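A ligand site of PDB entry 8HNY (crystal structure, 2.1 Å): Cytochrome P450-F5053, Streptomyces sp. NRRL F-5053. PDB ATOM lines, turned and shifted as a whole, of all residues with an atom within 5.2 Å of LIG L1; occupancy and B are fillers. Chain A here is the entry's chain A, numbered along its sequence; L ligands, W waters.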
ATOM      1  N   SER A  61       2.227  26.349  -7.800  1.00  0.00           N
ATOM      2  CA  SER A  61       2.765  25.247  -8.566  1.00  0.00           C
ATOM      3  C   SER A  61       3.487  25.728  -9.830  1.00  0.00           C
ATOM      4  O   SER A  61       4.614  25.292 -10.123  1.00  0.00           O
ATOM      5  CB  SER A  61       1.633  24.283  -8.950  1.00  0.00           C
ATOM      6  OG  SER A  61       2.012  23.599 -10.138  1.00  0.00           O
ATOM      7  N   ILE A  87      -0.513  22.688 -18.781  1.00  0.00           N
ATOM      8  CA  ILE A  87      -1.883  22.689 -18.262  1.00  0.00           C
ATOM      9  C   ILE A  87      -2.344  24.108 -17.936  1.00  0.00           C
ATOM     10  O   ILE A  87      -3.489  24.484 -18.207  1.00  0.00           O
ATOM     11  CB  ILE A  87      -2.009  21.746 -17.046  1.00  0.00           C
ATOM     12  CG1 ILE A  87      -3.476  21.373 -16.766  1.00  0.00           C
ATOM     13  CG2 ILE A  87      -1.414  22.377 -15.803  1.00  0.00           C
ATOM     14  CD1 ILE A  87      -4.176  20.586 -17.876  1.00  0.00           C
ATOM     15  N   ARG A  91      -5.476  25.801 -19.731  1.00  0.00           N
ATOM     16  CA  ARG A  91      -6.565  26.462 -19.012  1.00  0.00           C
ATOM     17  C   ARG A  91      -6.596  27.964 -19.316  1.00  0.00           C
ATOM     18  O   ARG A  91      -7.680  28.553 -19.406  1.00  0.00           O
ATOM     19  CB  ARG A  91      -6.455  26.229 -17.497  1.00  0.00           C
ATOM     20  CG  ARG A  91      -6.846  24.826 -17.025  1.00  0.00           C
ATOM     21  CD  ARG A  91      -6.330  24.494 -15.620  1.00  0.00           C
ATOM     22  NE  ARG A  91      -6.717  23.155 -15.210  1.00  0.00           N
ATOM     23  CZ  ARG A  91      -6.115  22.428 -14.274  1.00  0.00           C
ATOM     24  NH1 ARG A  91      -5.062  22.894 -13.609  1.00  0.00           N
ATOM     25  NH2 ARG A  91      -6.558  21.196 -14.014  1.00  0.00           N
ATOM     26  N   LEU A 103     -11.935  14.643 -20.229  1.00  0.00           N
ATOM     27  CA  LEU A 103     -11.488  13.951 -19.037  1.00  0.00           C
ATOM     28  C   LEU A 103     -12.593  13.715 -18.010  1.00  0.00           C
ATOM     29  O   LEU A 103     -12.357  12.961 -17.048  1.00  0.00           O
ATOM     30  CB  LEU A 103     -10.343  14.729 -18.370  1.00  0.00           C
ATOM     31  CG  LEU A 103      -9.143  15.027 -19.282  1.00  0.00           C
ATOM     32  CD1 LEU A 103      -8.288  16.116 -18.703  1.00  0.00           C
ATOM     33  CD2 LEU A 103      -8.301  13.769 -19.544  1.00  0.00           C
ATOM     34  N   LEU A 147      -5.487   3.172 -23.197  1.00  0.00           N
ATOM     35  CA  LEU A 147      -6.011   4.373 -22.561  1.00  0.00           C
ATOM     36  C   LEU A 147      -5.357   5.631 -23.133  1.00  0.00           C
ATOM     37  O   LEU A 147      -6.049   6.589 -23.508  1.00  0.00           O
ATOM     38  CB  LEU A 147      -5.811   4.322 -21.051  1.00  0.00           C
ATOM     39  CG  LEU A 147      -6.357   5.485 -20.236  1.00  0.00           C
ATOM     40  CD1 LEU A 147      -7.874   5.407 -20.119  1.00  0.00           C
ATOM     41  CD2 LEU A 147      -5.715   5.499 -18.852  1.00  0.00           C
ATOM     42  N   THR A 151      -8.022   7.593 -25.387  1.00  0.00           N
ATOM     43  CA  THR A 151      -8.625   8.736 -24.699  1.00  0.00           C
ATOM     44  C   THR A 151      -7.790  10.018 -24.720  1.00  0.00           C
ATOM     45  O   THR A 151      -8.349  11.103 -24.528  1.00  0.00           O
ATOM     46  CB  THR A 151      -8.920   8.390 -23.219  1.00  0.00           C
ATOM     47  OG1 THR A 151      -7.684   8.409 -22.477  1.00  0.00           O
ATOM     48  CG2 THR A 151      -9.628   7.005 -23.088  1.00  0.00           C
ATOM     49  N   LEU A 152      -6.481   9.947 -24.949  1.00  0.00           N
ATOM     50  CA  LEU A 152      -5.646  11.148 -24.830  1.00  0.00           C
ATOM     51  C   LEU A 152      -5.129  11.609 -26.187  1.00  0.00           C
ATOM     52  O   LEU A 152      -5.499  12.700 -26.636  1.00  0.00           O
ATOM     53  CB  LEU A 152      -4.487  10.896 -23.861  1.00  0.00           C
ATOM     54  CG  LEU A 152      -4.915  10.459 -22.449  1.00  0.00           C
ATOM     55  CD1 LEU A 152      -3.710  10.421 -21.530  1.00  0.00           C
ATOM     56  CD2 LEU A 152      -6.010  11.368 -21.885  1.00  0.00           C
ATOM     57  N   LEU A 233       2.671  16.897 -22.429  1.00  0.00           N
ATOM     58  CA  LEU A 233       2.054  16.920 -21.111  1.00  0.00           C
ATOM     59  C   LEU A 233       1.194  15.698 -20.887  1.00  0.00           C
ATOM     60  O   LEU A 233       1.235  15.091 -19.801  1.00  0.00           O
ATOM     61  CB  LEU A 233       1.215  18.188 -20.943  1.00  0.00           C
ATOM     62  CG  LEU A 233       0.115  18.091 -19.896  1.00  0.00           C
ATOM     63  CD1 LEU A 233       0.734  18.148 -18.516  1.00  0.00           C
ATOM     64  CD2 LEU A 233      -0.924  19.177 -20.065  1.00  0.00           C
ATOM     65  N   LEU A 234       0.406  15.292 -21.892  1.00  0.00           N
ATOM     66  CA  LEU A 234      -0.495  14.160 -21.699  1.00  0.00           C
ATOM     67  C   LEU A 234       0.285  12.848 -21.603  1.00  0.00           C
ATOM     68  O   LEU A 234      -0.128  11.942 -20.871  1.00  0.00           O
ATOM     69  CB  LEU A 234      -1.529  14.100 -22.820  1.00  0.00           C
ATOM     70  CG  LEU A 234      -2.377  15.353 -23.006  1.00  0.00           C
ATOM     71  CD1 LEU A 234      -3.156  15.264 -24.292  1.00  0.00           C
ATOM     72  CD2 LEU A 234      -3.343  15.603 -21.842  1.00  0.00           C
ATOM     73  N   ALA A 237       1.822  12.975 -17.892  1.00  0.00           N
ATOM     74  CA  ALA A 237       0.835  12.937 -16.811  1.00  0.00           C
ATOM     75  C   ALA A 237       0.027  11.648 -16.767  1.00  0.00           C
ATOM     76  O   ALA A 237      -0.502  11.301 -15.699  1.00  0.00           O
ATOM     77  CB  ALA A 237      -0.135  14.126 -16.954  1.00  0.00           C
ATOM     78  N   GLY A 238      -0.118  10.959 -17.899  1.00  0.00           N
ATOM     79  CA  GLY A 238      -1.047   9.857 -17.979  1.00  0.00           C
ATOM     80  C   GLY A 238      -0.449   8.527 -18.368  1.00  0.00           C
ATOM     81  O   GLY A 238      -1.061   7.479 -18.111  1.00  0.00           O
ATOM     82  N   THR A 241       2.315   7.316 -15.210  1.00  0.00           N
ATOM     83  CA  THR A 241       1.489   7.272 -14.006  1.00  0.00           C
ATOM     84  C   THR A 241       0.498   6.105 -14.051  1.00  0.00           C
ATOM     85  O   THR A 241       0.418   5.329 -13.098  1.00  0.00           O
ATOM     86  CB  THR A 241       0.730   8.587 -13.884  1.00  0.00           C
ATOM     87  OG1 THR A 241       0.178   8.924 -15.160  1.00  0.00           O
ATOM     88  CG2 THR A 241       1.673   9.687 -13.467  1.00  0.00           C
ATOM     89  N   SER A 242      -0.265   5.982 -15.138  1.00  0.00           N
ATOM     90  CA  SER A 242      -1.249   4.896 -15.230  1.00  0.00           C
ATOM     91  C   SER A 242      -0.555   3.538 -15.183  1.00  0.00           C
ATOM     92  O   SER A 242      -1.012   2.623 -14.493  1.00  0.00           O
ATOM     93  CB  SER A 242      -2.061   5.013 -16.513  1.00  0.00           C
ATOM     94  OG  SER A 242      -2.838   6.206 -16.530  1.00  0.00           O
ATOM     95  N   PHE A 245       0.953   2.882 -11.774  1.00  0.00           N
ATOM     96  CA  PHE A 245      -0.016   2.651 -10.710  1.00  0.00           C
ATOM     97  C   PHE A 245      -0.668   1.281 -10.849  1.00  0.00           C
ATOM     98  O   PHE A 245      -0.781   0.541  -9.867  1.00  0.00           O
ATOM     99  CB  PHE A 245      -1.102   3.719 -10.646  1.00  0.00           C
ATOM    100  CG  PHE A 245      -2.048   3.491  -9.503  1.00  0.00           C
ATOM    101  CD1 PHE A 245      -1.657   3.816  -8.218  1.00  0.00           C
ATOM    102  CD2 PHE A 245      -3.242   2.827  -9.692  1.00  0.00           C
ATOM    103  CE1 PHE A 245      -2.467   3.545  -7.147  1.00  0.00           C
ATOM    104  CE2 PHE A 245      -4.096   2.559  -8.628  1.00  0.00           C
ATOM    105  CZ  PHE A 245      -3.706   2.916  -7.346  1.00  0.00           C
ATOM    106  N   LEU A 278      -5.546   3.671  -4.047  1.00  0.00           N
ATOM    107  CA  LEU A 278      -4.953   4.986  -4.257  1.00  0.00           C
ATOM    108  C   LEU A 278      -4.310   5.538  -2.993  1.00  0.00           C
ATOM    109  O   LEU A 278      -3.395   6.369  -3.079  1.00  0.00           O
ATOM    110  CB  LEU A 278      -6.027   5.943  -4.766  1.00  0.00           C
ATOM    111  CG  LEU A 278      -6.474   5.674  -6.203  1.00  0.00           C
ATOM    112  CD1 LEU A 278      -7.775   6.401  -6.496  1.00  0.00           C
ATOM    113  CD2 LEU A 278      -5.341   6.066  -7.202  1.00  0.00           C
ATOM    114  N   LEU A 283       3.194   5.361  -5.523  1.00  0.00           N
ATOM    115  CA  LEU A 283       3.480   5.590  -6.931  1.00  0.00           C
ATOM    116  C   LEU A 283       4.751   6.416  -7.079  1.00  0.00           C
ATOM    117  O   LEU A 283       5.820   5.885  -7.399  1.00  0.00           O
ATOM    118  CB  LEU A 283       2.325   6.323  -7.617  1.00  0.00           C
ATOM    119  CG  LEU A 283       2.413   6.403  -9.141  1.00  0.00           C
ATOM    120  CD1 LEU A 283       2.271   5.008  -9.712  1.00  0.00           C
ATOM    121  CD2 LEU A 283       1.318   7.317  -9.685  1.00  0.00           C
ATOM    122  N   VAL A 288       5.015  16.200  -4.870  1.00  0.00           N
ATOM    123  CA  VAL A 288       4.433  17.372  -5.505  1.00  0.00           C
ATOM    124  C   VAL A 288       5.199  18.552  -4.943  1.00  0.00           C
ATOM    125  O   VAL A 288       5.731  18.498  -3.831  1.00  0.00           O
ATOM    126  CB  VAL A 288       2.931  17.521  -5.255  1.00  0.00           C
ATOM    127  CG1 VAL A 288       2.142  16.211  -5.542  1.00  0.00           C
ATOM    128  CG2 VAL A 288       2.732  17.994  -3.848  1.00  0.00           C
ATOM    129  N   LYS A 289       5.269  19.646  -5.702  1.00  0.00           N
ATOM    130  CA  LYS A 289       6.075  20.768  -5.218  1.00  0.00           C
ATOM    131  C   LYS A 289       5.431  22.097  -5.564  1.00  0.00           C
ATOM    132  O   LYS A 289       4.774  22.243  -6.597  1.00  0.00           O
ATOM    133  CB  LYS A 289       7.504  20.714  -5.789  1.00  0.00           C
ATOM    134  CG  LYS A 289       7.592  21.248  -7.185  1.00  0.00           C
ATOM    135  CD  LYS A 289       7.290  20.170  -8.191  1.00  0.00           C
ATOM    136  CE  LYS A 289       7.265  20.790  -9.577  1.00  0.00           C
ATOM    137  NZ  LYS A 289       6.459  19.933 -10.480  1.00  0.00           N
ATOM    138  N   ARG A 290       5.616  23.073  -4.676  1.00  0.00           N
ATOM    139  CA  ARG A 290       5.087  24.417  -4.838  1.00  0.00           C
ATOM    140  C   ARG A 290       6.117  25.422  -4.341  1.00  0.00           C
ATOM    141  O   ARG A 290       7.066  25.065  -3.634  1.00  0.00           O
ATOM    142  CB  ARG A 290       3.755  24.640  -4.075  1.00  0.00           C
ATOM    143  CG  ARG A 290       2.670  23.570  -4.262  1.00  0.00           C
ATOM    144  CD  ARG A 290       1.785  23.805  -5.507  1.00  0.00           C
ATOM    145  NE  ARG A 290       0.623  22.917  -5.522  1.00  0.00           N
ATOM    146  CZ  ARG A 290       0.622  21.685  -6.033  1.00  0.00           C
ATOM    147  NH1 ARG A 290       1.721  21.142  -6.535  1.00  0.00           N
ATOM    148  NH2 ARG A 290      -0.498  20.978  -6.040  1.00  0.00           N
ATOM    149  N   LEU A 313       3.140  12.570  -1.236  1.00  0.00           N
ATOM    150  CA  LEU A 313       1.832  11.964  -1.100  1.00  0.00           C
ATOM    151  C   LEU A 313       1.942  10.597  -0.446  1.00  0.00           C
ATOM    152  O   LEU A 313       1.066  10.199   0.327  1.00  0.00           O
ATOM    153  CB  LEU A 313       1.146  11.875  -2.457  1.00  0.00           C
ATOM    154  CG  LEU A 313       1.075  13.181  -3.264  1.00  0.00           C
ATOM    155  CD1 LEU A 313       0.393  12.988  -4.615  1.00  0.00           C
ATOM    156  CD2 LEU A 313       0.352  14.232  -2.455  1.00  0.00           C
ATOM    157  N   PHE A 339      -4.503  11.062  -0.637  1.00  0.00           N
ATOM    158  CA  PHE A 339      -3.718  12.010  -1.416  1.00  0.00           C
ATOM    159  C   PHE A 339      -3.199  11.427  -2.729  1.00  0.00           C
ATOM    160  O   PHE A 339      -2.391  12.063  -3.405  1.00  0.00           O
ATOM    161  CB  PHE A 339      -2.550  12.532  -0.569  1.00  0.00           C
ATOM    162  CG  PHE A 339      -2.912  13.740   0.234  1.00  0.00           C
ATOM    163  CD1 PHE A 339      -3.880  13.666   1.238  1.00  0.00           C
ATOM    164  CD2 PHE A 339      -2.304  14.974  -0.031  1.00  0.00           C
ATOM    165  CE1 PHE A 339      -4.234  14.802   1.990  1.00  0.00           C
ATOM    166  CE2 PHE A 339      -2.661  16.113   0.713  1.00  0.00           C
ATOM    167  CZ  PHE A 339      -3.617  16.027   1.720  1.00  0.00           C
ATOM    168  N   GLY A 340      -3.661  10.232  -3.106  1.00  0.00           N
ATOM    169  CA  GLY A 340      -3.200   9.613  -4.335  1.00  0.00           C
ATOM    170  C   GLY A 340      -3.316  10.470  -5.565  1.00  0.00           C
ATOM    171  O   GLY A 340      -2.551  10.309  -6.520  1.00  0.00           O
ATOM    172  N   PHE A 341      -4.281  11.388  -5.592  1.00  0.00           N
ATOM    173  CA  PHE A 341      -4.485  12.334  -6.689  1.00  0.00           C
ATOM    174  C   PHE A 341      -4.104  13.756  -6.299  1.00  0.00           C
ATOM    175  O   PHE A 341      -4.411  14.710  -7.034  1.00  0.00           O
ATOM    176  CB  PHE A 341      -5.953  12.288  -7.156  1.00  0.00           C
ATOM    177  CG  PHE A 341      -6.319  11.056  -7.954  1.00  0.00           C
ATOM    178  CD1 PHE A 341      -5.566  10.663  -9.067  1.00  0.00           C
ATOM    179  CD2 PHE A 341      -7.388  10.273  -7.577  1.00  0.00           C
ATOM    180  CE1 PHE A 341      -5.911   9.538  -9.793  1.00  0.00           C
ATOM    181  CE2 PHE A 341      -7.723   9.126  -8.301  1.00  0.00           C
ATOM    182  CZ  PHE A 341      -6.990   8.764  -9.411  1.00  0.00           C
ATOM    183  N   GLY A 342      -3.477  13.932  -5.139  1.00  0.00           N
ATOM    184  CA  GLY A 342      -3.202  15.273  -4.684  1.00  0.00           C
ATOM    185  C   GLY A 342      -4.358  15.844  -3.913  1.00  0.00           C
ATOM    186  O   GLY A 342      -5.042  15.126  -3.175  1.00  0.00           O
ATOM    187  N   ARG A 345      -6.552  22.891  -5.913  1.00  0.00           N
ATOM    188  CA  ARG A 345      -6.757  23.352  -7.283  1.00  0.00           C
ATOM    189  C   ARG A 345      -6.104  22.448  -8.325  1.00  0.00           C
ATOM    190  O   ARG A 345      -6.524  22.445  -9.484  1.00  0.00           O
ATOM    191  CB  ARG A 345      -6.226  24.784  -7.447  1.00  0.00           C
ATOM    192  CG  ARG A 345      -7.086  25.829  -6.717  1.00  0.00           C
ATOM    193  CD  ARG A 345      -6.668  27.243  -7.055  1.00  0.00           C
ATOM    194  NE  ARG A 345      -6.631  27.472  -8.497  1.00  0.00           N
ATOM    195  CZ  ARG A 345      -5.514  27.555  -9.200  1.00  0.00           C
ATOM    196  NH1 ARG A 345      -4.319  27.361  -8.645  1.00  0.00           N
ATOM    197  NH2 ARG A 345      -5.583  27.841 -10.502  1.00  0.00           N
ATOM    198  N   HIS A 346      -5.087  21.684  -7.936  1.00  0.00           N
ATOM    199  CA  HIS A 346      -4.355  20.868  -8.885  1.00  0.00           C
ATOM    200  C   HIS A 346      -4.692  19.398  -8.733  1.00  0.00           C
ATOM    201  O   HIS A 346      -3.922  18.527  -9.161  1.00  0.00           O
ATOM    202  CB  HIS A 346      -2.863  21.130  -8.760  1.00  0.00           C
ATOM    203  CG  HIS A 346      -2.492  22.573  -8.939  1.00  0.00           C
ATOM    204  ND1 HIS A 346      -2.381  23.145 -10.184  1.00  0.00           N
ATOM    205  CD2 HIS A 346      -2.218  23.551  -8.034  1.00  0.00           C
ATOM    206  CE1 HIS A 346      -2.061  24.430 -10.043  1.00  0.00           C
ATOM    207  NE2 HIS A 346      -1.949  24.697  -8.753  1.00  0.00           N
ATOM    208  N   PHE A 347      -5.844  19.101  -8.123  1.00  0.00           N
ATOM    209  CA  PHE A 347      -6.322  17.728  -8.056  1.00  0.00           C
ATOM    210  C   PHE A 347      -6.223  17.115  -9.456  1.00  0.00           C
ATOM    211  O   PHE A 347      -6.640  17.730 -10.440  1.00  0.00           O
ATOM    212  CB  PHE A 347      -7.765  17.704  -7.543  1.00  0.00           C
ATOM    213  CG  PHE A 347      -8.220  16.336  -7.076  1.00  0.00           C
ATOM    214  CD1 PHE A 347      -7.823  15.830  -5.837  1.00  0.00           C
ATOM    215  CD2 PHE A 347      -9.037  15.568  -7.870  1.00  0.00           C
ATOM    216  CE1 PHE A 347      -8.238  14.581  -5.408  1.00  0.00           C
ATOM    217  CE2 PHE A 347      -9.454  14.320  -7.450  1.00  0.00           C
ATOM    218  CZ  PHE A 347      -9.050  13.827  -6.221  1.00  0.00           C
ATOM    219  N   CYS A 348      -5.620  15.922  -9.537  1.00  0.00           N
ATOM    220  CA  CYS A 348      -5.414  15.336 -10.854  1.00  0.00           C
ATOM    221  C   CYS A 348      -6.678  15.380 -11.691  1.00  0.00           C
ATOM    222  O   CYS A 348      -7.662  14.664 -11.409  1.00  0.00           O
ATOM    223  CB  CYS A 348      -4.946  13.878 -10.765  1.00  0.00           C
ATOM    224  SG  CYS A 348      -5.008  12.959 -12.370  1.00  0.00           S
ATOM    225  N   PRO A 349      -6.687  16.157 -12.767  1.00  0.00           N
ATOM    226  CA  PRO A 349      -7.812  16.082 -13.704  1.00  0.00           C
ATOM    227  C   PRO A 349      -7.950  14.717 -14.366  1.00  0.00           C
ATOM    228  O   PRO A 349      -9.021  14.430 -14.908  1.00  0.00           O
ATOM    229  CB  PRO A 349      -7.478  17.159 -14.737  1.00  0.00           C
ATOM    230  CG  PRO A 349      -6.021  17.186 -14.741  1.00  0.00           C
ATOM    231  CD  PRO A 349      -5.565  16.925 -13.323  1.00  0.00           C
ATOM    232  N   GLY A 350      -6.888  13.899 -14.397  1.00  0.00           N
ATOM    233  CA  GLY A 350      -7.016  12.543 -14.921  1.00  0.00           C
ATOM    234  C   GLY A 350      -7.709  11.575 -13.971  1.00  0.00           C
ATOM    235  O   GLY A 350      -7.784  10.383 -14.269  1.00  0.00           O
ATOM    236  N   LEU A 353     -10.678   9.213 -15.486  1.00  0.00           N
ATOM    237  CA  LEU A 353     -10.237   8.169 -16.403  1.00  0.00           C
ATOM    238  C   LEU A 353      -9.330   7.166 -15.685  1.00  0.00           C
ATOM    239  O   LEU A 353      -9.371   5.960 -15.975  1.00  0.00           O
ATOM    240  CB  LEU A 353      -9.529   8.781 -17.600  1.00  0.00           C
ATOM    241  CG  LEU A 353     -10.390   9.440 -18.679  1.00  0.00           C
ATOM    242  CD1 LEU A 353      -9.506   9.956 -19.811  1.00  0.00           C
ATOM    243  CD2 LEU A 353     -11.430   8.482 -19.205  1.00  0.00           C
ATOM    244  N   ALA A 354      -8.510   7.646 -14.746  1.00  0.00           N
ATOM    245  CA  ALA A 354      -7.659   6.732 -14.001  1.00  0.00           C
ATOM    246  C   ALA A 354      -8.470   5.831 -13.098  1.00  0.00           C
ATOM    247  O   ALA A 354      -8.169   4.638 -12.962  1.00  0.00           O
ATOM    248  CB  ALA A 354      -6.625   7.502 -13.175  1.00  0.00           C
HETATM  249  C1  LIG L   1      -1.833  16.024 -11.734  1.00  0.00           C
HETATM  250  C2  LIG L   1      -3.460  14.341 -15.951  1.00  0.00           C
HETATM  251  C3  LIG L   1      -3.362   9.855 -14.193  1.00  0.00           C
HETATM  252  C4  LIG L   1      -1.949  11.589  -9.923  1.00  0.00           C
HETATM  253  C5  LIG L   1      -2.223  15.928 -13.040  1.00  0.00           C
HETATM  254  C6  LIG L   1      -2.217  17.024 -13.983  1.00  0.00           C
HETATM  255  C7  LIG L   1      -2.664  16.572 -15.142  1.00  0.00           C
HETATM  256  C8  LIG L   1      -2.966  15.158 -14.977  1.00  0.00           C
HETATM  257  C9  LIG L   1      -2.831  17.395 -16.439  1.00  0.00           C
HETATM  258  C10 LIG L   1      -1.769  18.462 -13.684  1.00  0.00           C
HETATM  259  C11 LIG L   1      -2.820  19.184 -12.834  1.00  0.00           C
HETATM  260  C12 LIG L   1      -2.277  20.531 -12.424  1.00  0.00           C
HETATM  261  O1  LIG L   1      -3.052  21.498 -12.441  1.00  0.00           O
HETATM  262  O2  LIG L   1      -1.057  20.638 -12.127  1.00  0.00           O
HETATM  263  C13 LIG L   1      -3.618  12.989 -15.824  1.00  0.00           C
HETATM  264  C14 LIG L   1      -4.076  12.101 -16.857  1.00  0.00           C
HETATM  265  C15 LIG L   1      -4.023  10.863 -16.360  1.00  0.00           C
HETATM  266  C16 LIG L   1      -3.538  10.934 -15.012  1.00  0.00           C
HETATM  267  C17 LIG L   1      -4.530  12.572 -18.259  1.00  0.00           C
HETATM  268  C18 LIG L   1      -4.459   9.541 -17.009  1.00  0.00           C
HETATM  269  C19 LIG L   1      -5.335   9.529 -18.015  1.00  0.00           C
HETATM  270  C20 LIG L   1      -2.935   9.922 -12.904  1.00  0.00           C
HETATM  271  C21 LIG L   1      -2.738   8.807 -12.015  1.00  0.00           C
HETATM  272  C22 LIG L   1      -2.351   9.280 -10.844  1.00  0.00           C
HETATM  273  C23 LIG L   1      -2.318  10.732 -10.932  1.00  0.00           C
HETATM  274  C24 LIG L   1      -2.929   7.294 -12.364  1.00  0.00           C
HETATM  275  C25 LIG L   1      -2.035   8.421  -9.609  1.00  0.00           C
HETATM  276  C26 LIG L   1      -1.344   8.909  -8.578  1.00  0.00           C
HETATM  277  C27 LIG L   1      -1.774  12.934 -10.024  1.00  0.00           C
HETATM  278  C28 LIG L   1      -1.382  13.842  -8.967  1.00  0.00           C
HETATM  279  C29 LIG L   1      -1.353  15.066  -9.470  1.00  0.00           C
HETATM  280  C30 LIG L   1      -1.746  14.979 -10.860  1.00  0.00           C
HETATM  281  C31 LIG L   1      -1.035  13.515  -7.501  1.00  0.00           C
HETATM  282  C32 LIG L   1      -1.000  16.341  -8.679  1.00  0.00           C
HETATM  283  C33 LIG L   1       0.408  16.856  -8.940  1.00  0.00           C
HETATM  284  C34 LIG L   1       0.553  18.177  -8.217  1.00  0.00           C
HETATM  285  O3  LIG L   1      -0.366  18.536  -7.426  1.00  0.00           O
HETATM  286  O4  LIG L   1       1.589  18.854  -8.427  1.00  0.00           O
HETATM  287  N1  LIG L   1      -2.686  14.798 -13.669  1.00  0.00           N
HETATM  288  N2  LIG L   1      -3.297  12.259 -14.710  1.00  0.00           N
HETATM  289  N3  LIG L   1      -2.682  11.079 -12.208  1.00  0.00           N
HETATM  290  N4  LIG L   1      -2.002  13.648 -11.179  1.00  0.00           N
HETATM  291 FE1  LIG L   1      -2.680  12.928 -12.889  1.00  0.00          FE
HETATM  292  C1  LG2 L   2       5.379  14.747  -9.362  1.00  0.00           C
HETATM  293  C2  LG2 L   2       4.223  15.185  -8.451  1.00  0.00           C
HETATM  294  C3  LG2 L   2       3.550  13.853  -8.051  1.00  0.00           C
HETATM  295  C4  LG2 L   2       3.685  13.190  -6.825  1.00  0.00           C
HETATM  296  C5  LG2 L   2       6.336  15.933  -9.537  1.00  0.00           C
HETATM  297  C6  LG2 L   2       8.086  14.299 -10.131  1.00  0.00           C
HETATM  298  C7  LG2 L   2       9.651  14.681  -9.679  1.00  0.00           C
HETATM  299  C8  LG2 L   2       9.824  16.186  -9.999  1.00  0.00           C
HETATM  300  C9  LG2 L   2       8.555  16.763 -10.080  1.00  0.00           C
HETATM  301  C10 LG2 L   2       7.516  13.201  -9.227  1.00  0.00           C
HETATM  302  C11 LG2 L   2       2.402  11.929  -8.162  1.00  0.00           C
HETATM  303  C12 LG2 L   2       1.589  10.899  -8.740  1.00  0.00           C
HETATM  304  C13 LG2 L   2       1.123  11.023 -10.048  1.00  0.00           C
HETATM  305  C14 LG2 L   2       1.475  12.163 -10.804  1.00  0.00           C
HETATM  306  C15 LG2 L   2       2.303  13.156 -10.250  1.00  0.00           C
HETATM  307  C16 LG2 L   2       2.758  13.035  -8.906  1.00  0.00           C
HETATM  308  F1  LG2 L   2       2.621  14.262 -10.983  1.00  0.00           F
HETATM  309  N1  LG2 L   2       7.549  15.432  -9.934  1.00  0.00           N
HETATM  310  N2  LG2 L   2       6.013  13.454  -8.802  1.00  0.00           N
HETATM  311  N3  LG2 L   2       2.982  12.048  -6.916  1.00  0.00           N
HETATM  312  O1  LG2 L   2       6.026  17.074  -9.384  1.00  0.00           O
HETATM  313  O2  LG2 L   2       8.154  12.223  -8.894  1.00  0.00           O
HETATM  314  O   HOH W   1      -2.742  18.066  -6.049  1.00  0.00           O
HETATM  315  O   HOH W   2      -0.081   8.465  -6.040  1.00  0.00           O
HETATM  316  O   HOH W   3       4.113  19.354  -8.325  1.00  0.00           O
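NH2 of Arg 290 lies within salt-bridge range of O3 of LIG L1 (2.8 Å). The side-chain sulfur (SG) of Cys 348 binds an iron atom (FE1) of LIG L1, 2.4 Å away. NH1 of Arg 91 lies within salt-bridge range of O1 of LIG L1, at 2.7 Å. ND1 of His 346 is in hydrogen-bond range of O1 of LIG L1 (2.9 Å). NZ of Lys 289 lies within hydrogen-bond range of O1 of LG2 L2.
O of Phe 341 lies within hydrogen-bond range of N of Cys 348 (3.0 Å). N of Gly 350 sits close to SG of Cys 348 (2.9 Å). O of Gly 238 lies within hydrogen-bond range of OG of Ser 242 (2.7 Å). OG1 of Thr 241 sits close to N of Gly 238 (3.4 Å). The side-chain hydroxyl (OG1) of Thr 241 sits at hydrogen-bond distance from the backbone carbonyl oxygen (O) of Ala 237 (2.5 Å).
The backbone carbonyl oxygen of Ala 237 sits close to a nitrogen (N2) of LIG L1 (3.1 Å). Ile 87 touches LIG L1 (CD1 to C9, 3.7 Å). Leu 152 touches LIG L1. Gly 238 touches LIG L1. OG1 of Thr 241 touches C3 of LIG L1, 3.8 Å away. Ser 242 touches LIG L1. CD2 of Leu 283 touches C26 of LIG L1, at 3.3 Å. Val 288 touches LIG L1 (CG1 to C34, 3.7 Å). Leu 313 touches LIG L1 (CD1 to C31, 3.3 Å). Gly 340 touches LIG L1 (O to C26, 2.8 Å). Phe 341 touches LIG L1 (C to C31, 3.3 Å). Gly 342 touches LIG L1 (N to C31, 3.4 Å). CD of Pro 349 touches C6 of LIG L1, at 3.4 Å. Gly 350 touches LIG L1. CB of Ala 354 touches C24 of LIG L1, at 3.8 Å. Hydrophobic or aromatic side chains that line LIG L1: Ile 87, Leu 152, Ala 237, Leu 283, Val 288, Leu 313, Phe 341, His 346, Pro 349 and Ala 354. The nearest printed residue that does not touch LIG L1 is Leu 147 (4.1 Å).
Water W3 lies within hydrogen-bond range of an oxygen (O4) of LIG L1 (2.6 Å), the backbone NH of Lys 289 (2.9 Å), an oxygen (O1) of LG2 L2 (3.2 Å) and the guanidinium group of Arg 290 (3.5 Å). Water W1 bridges O3 of LIG L1 and O of His 346.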
